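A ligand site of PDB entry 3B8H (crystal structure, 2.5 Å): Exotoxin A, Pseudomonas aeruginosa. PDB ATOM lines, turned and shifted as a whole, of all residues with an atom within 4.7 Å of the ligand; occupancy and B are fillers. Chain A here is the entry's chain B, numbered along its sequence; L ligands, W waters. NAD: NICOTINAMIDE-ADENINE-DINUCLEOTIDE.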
ATOM      1  N   TYR A  41     -25.357   4.151 -23.336  1.00  0.00           N
ATOM      2  CA  TYR A  41     -25.049   5.572 -23.434  1.00  0.00           C
ATOM      3  C   TYR A  41     -24.279   6.081 -22.224  1.00  0.00           C
ATOM      4  O   TYR A  41     -24.396   5.552 -21.124  1.00  0.00           O
ATOM      5  CB  TYR A  41     -26.342   6.385 -23.567  1.00  0.00           C
ATOM      6  CG  TYR A  41     -27.057   6.222 -24.878  1.00  0.00           C
ATOM      7  CD1 TYR A  41     -26.805   7.086 -25.943  1.00  0.00           C
ATOM      8  CD2 TYR A  41     -28.003   5.220 -25.053  1.00  0.00           C
ATOM      9  CE1 TYR A  41     -27.461   6.948 -27.149  1.00  0.00           C
ATOM     10  CE2 TYR A  41     -28.670   5.074 -26.265  1.00  0.00           C
ATOM     11  CZ  TYR A  41     -28.402   5.936 -27.305  1.00  0.00           C
ATOM     12  OH  TYR A  41     -29.056   5.791 -28.504  1.00  0.00           O
ATOM     13  N   HIS A  42     -23.492   7.142 -22.438  1.00  0.00           N
ATOM     14  CA  HIS A  42     -22.824   7.838 -21.350  1.00  0.00           C
ATOM     15  C   HIS A  42     -22.959   9.338 -21.544  1.00  0.00           C
ATOM     16  O   HIS A  42     -22.517   9.882 -22.552  1.00  0.00           O
ATOM     17  CB  HIS A  42     -21.344   7.447 -21.275  1.00  0.00           C
ATOM     18  CG  HIS A  42     -20.578   8.194 -20.226  1.00  0.00           C
ATOM     19  ND1 HIS A  42     -20.389   7.712 -18.956  1.00  0.00           N
ATOM     20  CD2 HIS A  42     -19.951   9.397 -20.271  1.00  0.00           C
ATOM     21  CE1 HIS A  42     -19.679   8.582 -18.255  1.00  0.00           C
ATOM     22  NE2 HIS A  42     -19.402   9.612 -19.030  1.00  0.00           N
ATOM     23  N   GLY A  43     -23.588  10.001 -20.582  1.00  0.00           N
ATOM     24  CA  GLY A  43     -23.727  11.449 -20.627  1.00  0.00           C
ATOM     25  C   GLY A  43     -22.696  12.131 -19.741  1.00  0.00           C
ATOM     26  O   GLY A  43     -22.408  11.663 -18.635  1.00  0.00           O
ATOM     27  N   THR A  44     -22.134  13.229 -20.230  1.00  0.00           N
ATOM     28  CA  THR A  44     -21.107  13.946 -19.492  1.00  0.00           C
ATOM     29  C   THR A  44     -20.922  15.351 -20.052  1.00  0.00           C
ATOM     30  O   THR A  44     -21.662  15.770 -20.934  1.00  0.00           O
ATOM     31  CB  THR A  44     -19.756  13.188 -19.542  1.00  0.00           C
ATOM     32  OG1 THR A  44     -18.850  13.754 -18.588  1.00  0.00           O
ATOM     33  CG2 THR A  44     -19.152  13.268 -20.933  1.00  0.00           C
ATOM     34  N   PHE A  45     -19.937  16.077 -19.515  1.00  0.00           N
ATOM     35  CA  PHE A  45     -19.674  17.438 -19.978  1.00  0.00           C
ATOM     36  C   PHE A  45     -18.748  17.473 -21.187  1.00  0.00           C
ATOM     37  O   PHE A  45     -18.077  16.496 -21.494  1.00  0.00           O
ATOM     38  CB  PHE A  45     -19.135  18.321 -18.841  1.00  0.00           C
ATOM     39  CG  PHE A  45     -17.921  17.763 -18.157  1.00  0.00           C
ATOM     40  CD1 PHE A  45     -18.027  16.706 -17.268  1.00  0.00           C
ATOM     41  CD2 PHE A  45     -16.674  18.320 -18.378  1.00  0.00           C
ATOM     42  CE1 PHE A  45     -16.912  16.199 -16.631  1.00  0.00           C
ATOM     43  CE2 PHE A  45     -15.548  17.821 -17.736  1.00  0.00           C
ATOM     44  CZ  PHE A  45     -15.668  16.757 -16.866  1.00  0.00           C
ATOM     45  N   ALA A  48     -15.087  16.352 -21.111  1.00  0.00           N
ATOM     46  CA  ALA A  48     -15.047  14.924 -20.826  1.00  0.00           C
ATOM     47  C   ALA A  48     -15.307  14.131 -22.102  1.00  0.00           C
ATOM     48  O   ALA A  48     -14.637  13.137 -22.381  1.00  0.00           O
ATOM     49  CB  ALA A  48     -16.055  14.563 -19.742  1.00  0.00           C
ATOM     50  N   SER A  51     -12.314  14.112 -24.226  1.00  0.00           N
ATOM     51  CA  SER A  51     -11.296  13.203 -23.687  1.00  0.00           C
ATOM     52  C   SER A  51     -11.629  11.749 -23.993  1.00  0.00           C
ATOM     53  O   SER A  51     -10.763  10.968 -24.376  1.00  0.00           O
ATOM     54  CB  SER A  51     -11.154  13.406 -22.179  1.00  0.00           C
ATOM     55  OG  SER A  51     -10.173  12.549 -21.629  1.00  0.00           O
ATOM     56  N   ILE A  52     -12.903  11.401 -23.815  1.00  0.00           N
ATOM     57  CA  ILE A  52     -13.341  10.020 -23.976  1.00  0.00           C
ATOM     58  C   ILE A  52     -13.324   9.559 -25.437  1.00  0.00           C
ATOM     59  O   ILE A  52     -12.900   8.445 -25.738  1.00  0.00           O
ATOM     60  CB  ILE A  52     -14.759   9.820 -23.386  1.00  0.00           C
ATOM     61  CG1 ILE A  52     -14.707   9.960 -21.856  1.00  0.00           C
ATOM     62  CG2 ILE A  52     -15.321   8.471 -23.786  1.00  0.00           C
ATOM     63  CD1 ILE A  52     -16.061  10.198 -21.208  1.00  0.00           C
ATOM     64  N   GLY A  56      -9.842   8.023 -25.363  1.00  0.00           N
ATOM     65  CA  GLY A  56     -10.342   6.763 -24.834  1.00  0.00           C
ATOM     66  C   GLY A  56     -10.776   6.876 -23.384  1.00  0.00           C
ATOM     67  O   GLY A  56     -10.353   7.774 -22.656  1.00  0.00           O
ATOM     68  N   VAL A  57     -11.621   5.944 -22.959  1.00  0.00           N
ATOM     69  CA  VAL A  57     -12.041   5.865 -21.571  1.00  0.00           C
ATOM     70  C   VAL A  57     -10.857   5.427 -20.697  1.00  0.00           C
ATOM     71  O   VAL A  57     -10.256   4.392 -20.935  1.00  0.00           O
ATOM     72  CB  VAL A  57     -13.194   4.859 -21.398  1.00  0.00           C
ATOM     73  CG1 VAL A  57     -13.421   4.543 -19.932  1.00  0.00           C
ATOM     74  CG2 VAL A  57     -14.461   5.399 -22.051  1.00  0.00           C
ATOM     75  N   ARG A  58     -10.522   6.243 -19.696  1.00  0.00           N
ATOM     76  CA  ARG A  58      -9.427   5.919 -18.780  1.00  0.00           C
ATOM     77  C   ARG A  58      -9.847   5.960 -17.310  1.00  0.00           C
ATOM     78  O   ARG A  58     -10.624   6.820 -16.895  1.00  0.00           O
ATOM     79  CB  ARG A  58      -8.220   6.830 -19.008  1.00  0.00           C
ATOM     80  CG  ARG A  58      -7.234   6.310 -20.041  1.00  0.00           C
ATOM     81  CD  ARG A  58      -7.708   6.559 -21.458  1.00  0.00           C
ATOM     82  NE  ARG A  58      -6.806   5.973 -22.443  1.00  0.00           N
ATOM     83  CZ  ARG A  58      -7.078   4.892 -23.159  1.00  0.00           C
ATOM     84  NH1 ARG A  58      -8.239   4.268 -23.020  1.00  0.00           N
ATOM     85  NH2 ARG A  58      -6.188   4.429 -24.023  1.00  0.00           N
ATOM     86  N   ARG A  60     -10.152   6.447 -13.327  1.00  0.00           N
ATOM     87  CA  ARG A  60      -9.982   7.625 -12.487  1.00  0.00           C
ATOM     88  C   ARG A  60     -10.683   7.418 -11.151  1.00  0.00           C
ATOM     89  O   ARG A  60     -11.535   6.539 -11.032  1.00  0.00           O
ATOM     90  CB  ARG A  60     -10.552   8.862 -13.182  1.00  0.00           C
ATOM     91  CG  ARG A  60     -12.054   8.775 -13.443  1.00  0.00           C
ATOM     92  CD  ARG A  60     -12.490   9.686 -14.569  1.00  0.00           C
ATOM     93  NE  ARG A  60     -11.578   9.612 -15.711  1.00  0.00           N
ATOM     94  CZ  ARG A  60     -10.769  10.591 -16.081  1.00  0.00           C
ATOM     95  NH1 ARG A  60     -10.766  11.746 -15.418  1.00  0.00           N
ATOM     96  NH2 ARG A  60      -9.971  10.437 -17.133  1.00  0.00           N
ATOM     97  N   GLN A  62     -13.302   8.036  -8.240  1.00  0.00           N
ATOM     98  CA  GLN A  62     -14.696   8.470  -8.214  1.00  0.00           C
ATOM     99  C   GLN A  62     -15.272   8.362  -6.803  1.00  0.00           C
ATOM    100  O   GLN A  62     -14.763   7.593  -5.986  1.00  0.00           O
ATOM    101  CB  GLN A  62     -15.527   7.660  -9.219  1.00  0.00           C
ATOM    102  CG  GLN A  62     -15.177   6.189  -9.264  1.00  0.00           C
ATOM    103  CD  GLN A  62     -15.555   5.529 -10.577  1.00  0.00           C
ATOM    104  OE1 GLN A  62     -15.155   4.402 -10.852  1.00  0.00           O
ATOM    105  NE2 GLN A  62     -16.332   6.231 -11.393  1.00  0.00           N
ATOM    106  N   LEU A  64     -17.334   6.939  -4.483  1.00  0.00           N
ATOM    107  CA  LEU A  64     -18.143   5.785  -4.083  1.00  0.00           C
ATOM    108  C   LEU A  64     -17.229   4.758  -3.423  1.00  0.00           C
ATOM    109  O   LEU A  64     -16.030   4.993  -3.290  1.00  0.00           O
ATOM    110  CB  LEU A  64     -18.877   5.179  -5.280  1.00  0.00           C
ATOM    111  CG  LEU A  64     -18.198   5.188  -6.657  1.00  0.00           C
ATOM    112  CD1 LEU A  64     -16.885   4.432  -6.640  1.00  0.00           C
ATOM    113  CD2 LEU A  64     -19.133   4.607  -7.715  1.00  0.00           C
ATOM    114  N   GLY A  70     -15.912   1.890 -11.644  1.00  0.00           N
ATOM    115  CA  GLY A  70     -16.002   1.500 -13.026  1.00  0.00           C
ATOM    116  C   GLY A  70     -16.614   2.597 -13.875  1.00  0.00           C
ATOM    117  O   GLY A  70     -16.876   3.697 -13.392  1.00  0.00           O
ATOM    118  N   PHE A  71     -16.856   2.285 -15.139  1.00  0.00           N
ATOM    119  CA  PHE A  71     -17.425   3.252 -16.066  1.00  0.00           C
ATOM    120  C   PHE A  71     -18.930   3.042 -16.169  1.00  0.00           C
ATOM    121  O   PHE A  71     -19.390   1.978 -16.583  1.00  0.00           O
ATOM    122  CB  PHE A  71     -16.757   3.130 -17.435  1.00  0.00           C
ATOM    123  CG  PHE A  71     -17.072   4.263 -18.366  1.00  0.00           C
ATOM    124  CD1 PHE A  71     -16.656   5.549 -18.071  1.00  0.00           C
ATOM    125  CD2 PHE A  71     -17.770   4.031 -19.541  1.00  0.00           C
ATOM    126  CE1 PHE A  71     -16.945   6.599 -18.934  1.00  0.00           C
ATOM    127  CE2 PHE A  71     -18.057   5.074 -20.399  1.00  0.00           C
ATOM    128  CZ  PHE A  71     -17.651   6.358 -20.101  1.00  0.00           C
ATOM    129  N   TYR A  72     -19.688   4.073 -15.796  1.00  0.00           N
ATOM    130  CA  TYR A  72     -21.139   3.958 -15.721  1.00  0.00           C
ATOM    131  C   TYR A  72     -21.831   4.417 -16.995  1.00  0.00           C
ATOM    132  O   TYR A  72     -21.589   5.527 -17.481  1.00  0.00           O
ATOM    133  CB  TYR A  72     -21.673   4.729 -14.517  1.00  0.00           C
ATOM    134  CG  TYR A  72     -21.406   4.064 -13.191  1.00  0.00           C
ATOM    135  CD1 TYR A  72     -20.120   4.004 -12.671  1.00  0.00           C
ATOM    136  CD2 TYR A  72     -22.436   3.507 -12.451  1.00  0.00           C
ATOM    137  CE1 TYR A  72     -19.862   3.393 -11.455  1.00  0.00           C
ATOM    138  CE2 TYR A  72     -22.199   2.900 -11.236  1.00  0.00           C
ATOM    139  CZ  TYR A  72     -20.909   2.845 -10.746  1.00  0.00           C
ATOM    140  OH  TYR A  72     -20.672   2.238  -9.532  1.00  0.00           O
ATOM    141  N   ILE A  73     -22.672   3.550 -17.530  1.00  0.00           N
ATOM    142  CA  ILE A  73     -23.460   3.866 -18.716  1.00  0.00           C
ATOM    143  C   ILE A  73     -24.884   3.369 -18.517  1.00  0.00           C
ATOM    144  O   ILE A  73     -25.168   2.676 -17.540  1.00  0.00           O
ATOM    145  CB  ILE A  73     -22.871   3.208 -19.980  1.00  0.00           C
ATOM    146  CG1 ILE A  73     -22.911   1.680 -19.853  1.00  0.00           C
ATOM    147  CG2 ILE A  73     -21.444   3.696 -20.223  1.00  0.00           C
ATOM    148  CD1 ILE A  73     -22.420   0.950 -21.088  1.00  0.00           C
ATOM    149  N   ALA A  74     -25.767   3.739 -19.424  1.00  0.00           N
ATOM    150  CA  ALA A  74     -27.164   3.314 -19.342  1.00  0.00           C
ATOM    151  C   ALA A  74     -27.692   2.966 -20.722  1.00  0.00           C
ATOM    152  O   ALA A  74     -27.409   3.660 -21.699  1.00  0.00           O
ATOM    153  CB  ALA A  74     -28.010   4.407 -18.699  1.00  0.00           C
ATOM    154  N   LEU A  79     -31.764   8.223 -19.261  1.00  0.00           N
ATOM    155  CA  LEU A  79     -31.073   8.164 -17.970  1.00  0.00           C
ATOM    156  C   LEU A  79     -29.724   8.854 -18.049  1.00  0.00           C
ATOM    157  O   LEU A  79     -29.406   9.725 -17.251  1.00  0.00           O
ATOM    158  CB  LEU A  79     -30.913   6.717 -17.509  1.00  0.00           C
ATOM    159  CG  LEU A  79     -30.071   6.499 -16.240  1.00  0.00           C
ATOM    160  CD1 LEU A  79     -30.630   7.300 -15.087  1.00  0.00           C
ATOM    161  CD2 LEU A  79     -30.009   5.016 -15.885  1.00  0.00           C
ATOM    162  N   ALA A  80     -28.921   8.458 -19.042  1.00  0.00           N
ATOM    163  CA  ALA A  80     -27.602   9.037 -19.247  1.00  0.00           C
ATOM    164  C   ALA A  80     -27.695  10.531 -19.544  1.00  0.00           C
ATOM    165  O   ALA A  80     -26.760  11.295 -19.284  1.00  0.00           O
ATOM    166  CB  ALA A  80     -26.885   8.316 -20.377  1.00  0.00           C
ATOM    167  N   TYR A  83     -27.022  13.279 -16.911  1.00  0.00           N
ATOM    168  CA  TYR A  83     -25.639  13.537 -16.510  1.00  0.00           C
ATOM    169  C   TYR A  83     -24.881  14.317 -17.574  1.00  0.00           C
ATOM    170  O   TYR A  83     -23.719  14.684 -17.379  1.00  0.00           O
ATOM    171  CB  TYR A  83     -24.921  12.223 -16.208  1.00  0.00           C
ATOM    172  CG  TYR A  83     -25.600  11.381 -15.152  1.00  0.00           C
ATOM    173  CD1 TYR A  83     -25.393  11.616 -13.807  1.00  0.00           C
ATOM    174  CD2 TYR A  83     -26.477  10.355 -15.510  1.00  0.00           C
ATOM    175  CE1 TYR A  83     -26.020  10.862 -12.841  1.00  0.00           C
ATOM    176  CE2 TYR A  83     -27.104   9.595 -14.553  1.00  0.00           C
ATOM    177  CZ  TYR A  83     -26.880   9.840 -13.218  1.00  0.00           C
ATOM    178  OH  TYR A  83     -27.507   9.086 -12.252  1.00  0.00           O
ATOM    179  N   GLU A 155     -28.942   0.628 -15.153  1.00  0.00           N
ATOM    180  CA  GLU A 155     -27.625   1.179 -15.440  1.00  0.00           C
ATOM    181  C   GLU A 155     -26.655   0.028 -15.664  1.00  0.00           C
ATOM    182  O   GLU A 155     -26.888  -1.093 -15.196  1.00  0.00           O
ATOM    183  CB  GLU A 155     -27.134   2.061 -14.285  1.00  0.00           C
ATOM    184  CG  GLU A 155     -26.763   1.294 -13.026  1.00  0.00           C
ATOM    185  CD  GLU A 155     -26.292   2.199 -11.901  1.00  0.00           C
ATOM    186  OE1 GLU A 155     -26.018   3.391 -12.170  1.00  0.00           O
ATOM    187  OE2 GLU A 155     -26.190   1.720 -10.757  1.00  0.00           O
ATOM    188  N   TRP A 160     -13.306  -1.298 -14.915  1.00  0.00           N
ATOM    189  CA  TRP A 160     -12.328  -0.390 -15.515  1.00  0.00           C
ATOM    190  C   TRP A 160     -11.469  -1.034 -16.604  1.00  0.00           C
ATOM    191  O   TRP A 160     -11.260  -0.435 -17.652  1.00  0.00           O
ATOM    192  CB  TRP A 160     -11.467   0.295 -14.447  1.00  0.00           C
ATOM    193  CG  TRP A 160     -12.115   1.510 -13.858  1.00  0.00           C
ATOM    194  CD1 TRP A 160     -12.368   1.751 -12.546  1.00  0.00           C
ATOM    195  CD2 TRP A 160     -12.605   2.658 -14.577  1.00  0.00           C
ATOM    196  NE1 TRP A 160     -12.979   2.972 -12.385  1.00  0.00           N
ATOM    197  CE2 TRP A 160     -13.143   3.547 -13.617  1.00  0.00           C
ATOM    198  CE3 TRP A 160     -12.648   3.015 -15.925  1.00  0.00           C
ATOM    199  CZ2 TRP A 160     -13.704   4.770 -13.974  1.00  0.00           C
ATOM    200  CZ3 TRP A 160     -13.208   4.224 -16.283  1.00  0.00           C
ATOM    201  CH2 TRP A 160     -13.729   5.092 -15.306  1.00  0.00           C
HETATM  202  PA  NAD L   1     -17.989   9.449 -12.281  1.00  0.00           P
HETATM  203  O1A NAD L   1     -17.524  10.101 -11.008  1.00  0.00           O
HETATM  204  O2A NAD L   1     -18.268   7.957 -12.296  1.00  0.00           O
HETATM  205  O5B NAD L   1     -16.864   9.774 -13.372  1.00  0.00           O
HETATM  206  C5B NAD L   1     -16.313  11.077 -13.364  1.00  0.00           C
HETATM  207  C4B NAD L   1     -16.277  11.738 -14.726  1.00  0.00           C
HETATM  208  O4B NAD L   1     -15.027  11.620 -15.400  1.00  0.00           O
HETATM  209  C3B NAD L   1     -17.341  11.241 -15.699  1.00  0.00           C
HETATM  210  O3B NAD L   1     -18.330  12.238 -15.882  1.00  0.00           O
HETATM  211  C2B NAD L   1     -16.621  11.054 -17.005  1.00  0.00           C
HETATM  212  O2B NAD L   1     -17.398  11.617 -18.072  1.00  0.00           O
HETATM  213  C1B NAD L   1     -15.345  11.853 -16.764  1.00  0.00           C
HETATM  214  N9A NAD L   1     -14.259  11.576 -17.749  1.00  0.00           N
HETATM  215  C8A NAD L   1     -13.576  12.513 -18.414  1.00  0.00           C
HETATM  216  N7A NAD L   1     -12.664  11.916 -19.206  1.00  0.00           N
HETATM  217  C5A NAD L   1     -12.781  10.587 -19.018  1.00  0.00           C
HETATM  218  C6A NAD L   1     -12.120   9.497 -19.556  1.00  0.00           C
HETATM  219  N6A NAD L   1     -11.134   9.673 -20.470  1.00  0.00           N
HETATM  220  N1A NAD L   1     -12.481   8.252 -19.143  1.00  0.00           N
HETATM  221  C2A NAD L   1     -13.451   8.079 -18.247  1.00  0.00           C
HETATM  222  N3A NAD L   1     -14.107   9.121 -17.721  1.00  0.00           N
HETATM  223  C4A NAD L   1     -13.780  10.379 -18.090  1.00  0.00           C
HETATM  224  O3  NAD L   1     -19.296  10.210 -12.828  1.00  0.00           O
HETATM  225  PN  NAD L   1     -20.415   9.508 -13.755  1.00  0.00           P
HETATM  226  O1N NAD L   1     -19.757   8.556 -14.724  1.00  0.00           O
HETATM  227  O2N NAD L   1     -21.325  10.584 -14.259  1.00  0.00           O
HETATM  228  O5D NAD L   1     -21.205   8.635 -12.662  1.00  0.00           O
HETATM  229  C5D NAD L   1     -21.897   9.295 -11.601  1.00  0.00           C
HETATM  230  C4D NAD L   1     -23.096   8.471 -11.172  1.00  0.00           C
HETATM  231  O4D NAD L   1     -24.113   8.563 -12.174  1.00  0.00           O
HETATM  232  C3D NAD L   1     -22.776   7.003 -11.007  1.00  0.00           C
HETATM  233  O3D NAD L   1     -22.555   6.671  -9.630  1.00  0.00           O
HETATM  234  C2D NAD L   1     -23.999   6.284 -11.544  1.00  0.00           C
HETATM  235  O2D NAD L   1     -24.781   5.805 -10.444  1.00  0.00           O
HETATM  236  C1D NAD L   1     -24.809   7.326 -12.290  1.00  0.00           C
HETATM  237  N1N NAD L   1     -24.926   6.981 -13.721  1.00  0.00           N
HETATM  238  C2N NAD L   1     -24.334   7.769 -14.633  1.00  0.00           C
HETATM  239  C3N NAD L   1     -24.435   7.484 -15.997  1.00  0.00           C
HETATM  240  C7N NAD L   1     -23.764   8.377 -17.004  1.00  0.00           C
HETATM  241  O7N NAD L   1     -24.163   8.379 -18.166  1.00  0.00           O
HETATM  242  N7N NAD L   1     -22.766   9.170 -16.617  1.00  0.00           N
HETATM  243  C4N NAD L   1     -25.157   6.382 -16.409  1.00  0.00           C
HETATM  244  C5N NAD L   1     -25.767   5.579 -15.444  1.00  0.00           C
HETATM  245  C6N NAD L   1     -25.645   5.911 -14.095  1.00  0.00           C
HETATM  246  O   HOH W   1     -25.001   3.601  -8.563  1.00  0.00           O
HETATM  247  O   HOH W   2     -17.956   6.663 -14.915  1.00  0.00           O
HETATM  248  O   HOH W   3      -8.342  10.030 -22.514  1.00  0.00           O
HETATM  249  O   HOH W   4     -20.888  12.070 -16.482  1.00  0.00           O
HETATM  250  O   HOH W   5      -9.460  13.046 -18.514  1.00  0.00           O
HETATM  251  O   HOH W   6     -19.451   7.259  -9.758  1.00  0.00           O
HETATM  252  O   HOH W   7     -21.649  12.868 -12.502  1.00  0.00           O
HETATM  253  O   HOH W   8     -19.134  12.528 -10.982  1.00  0.00           O
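A nitrogen (N3A) of the ligand sits at hydrogen-bond distance from the guanidinium group of Arg 60, 3.3 Å away. O7N of the ligand is in hydrogen-bond range of N of Gly 43 (3.0 Å). O2B of the ligand lies within hydrogen-bond range of NE2 of His 42 (3.0 Å). O of Gly 56 is in hydrogen-bond range of N6A of the ligand, at 3.0 Å. The backbone NH of Arg 58 sits at hydrogen-bond distance from a nitrogen (N1A) of the ligand, 2.9 Å away. O of Gly 43 lies within hydrogen-bond range of N7N of the ligand (3.2 Å). OG of Ser 51 sits at hydrogen-bond distance from N6A of the ligand (3.2 Å). The side-chain hydroxyl of Thr 44 sits at hydrogen-bond distance from an oxygen (O2B) of the ligand (2.6 Å). The side-chain hydroxyl of Tyr 83 lies close to an oxygen (O4D) of the ligand (3.4 Å). O2D of the ligand lies close to OE1 of Glu 155, at 3.2 Å. An oxygen (O2A) of the ligand is in hydrogen-bond range of the side-chain amide nitrogen (NE2) of Gln 62 (2.7 Å).
The backbone NH of Gly 70 sits at hydrogen-bond distance from the side-chain amide oxygen of Gln 62, at 2.7 Å. The backbone NH (N) of Gly 56 is in hydrogen-bond range of the backbone carbonyl oxygen (O) of Ser 51 (3.2 Å). NE of Arg 60 sits at hydrogen-bond distance from O of Arg 58. O of Tyr 72 sits at hydrogen-bond distance from ND1 of His 42 (2.9 Å). OE1 of Gln 62 lies within hydrogen-bond range of NE1 of Trp 160.
Ala 48 touches the ligand (CB to C8A, 3.5 Å). CG1 of Ile 52 touches C5A of the ligand (3.5 Å). Val 57 touches the ligand. Phe 71 touches the ligand (CE1 to C2A, 3.9 Å). Tyr 72 touches the ligand (CD2 to C2D, 3.3 Å). Ile 73 touches the ligand (O to C5N, 3.6 Å). CB of Ala 80 touches O7N of the ligand (3.5 Å). Hydrophobic or aromatic side chains within 4 Å of the ligand: His 42, Ala 48, Ile 52, Val 57, Phe 71, Tyr 72, Ala 80 and Tyr 83. Within 4 Å of the ligand: His 42, Gly 43, Thr 44, Ala 48, Ser 51, Ile 52, Gly 56, Val 57, Arg 58, Arg 60, Gln 62, Phe 71, Tyr 72, Ile 73, Ala 80, Tyr 83 and Glu 155. The nearest printed residue that does not touch the ligand is Ala 74 (4.1 Å).
Water W2 lies within hydrogen-bond range of O1N of the ligand (2.6 Å) and N of Tyr 72 (3.2 Å). Water W4 lies within hydrogen-bond range of an oxygen (O3B) of the ligand (2.6 Å), the backbone carbonyl oxygen (O) of Gly 43 (2.7 Å) and the side-chain hydroxyl (OG1) of Thr 44 (3.4 Å). Water W1 bridges O2D of the ligand (2.9 Å) and OE2 of Glu 155 (3.1 Å). Water W5 lies within hydrogen-bond range of NH2 of Arg 60, OG of Ser 51 and N7A of the ligand. Water W3 lies within hydrogen-bond range of the backbone carbonyl oxygen (O) of Gly 56, the backbone carbonyl oxygen (O) of Ser 51 and a nitrogen (N6A) of the ligand.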
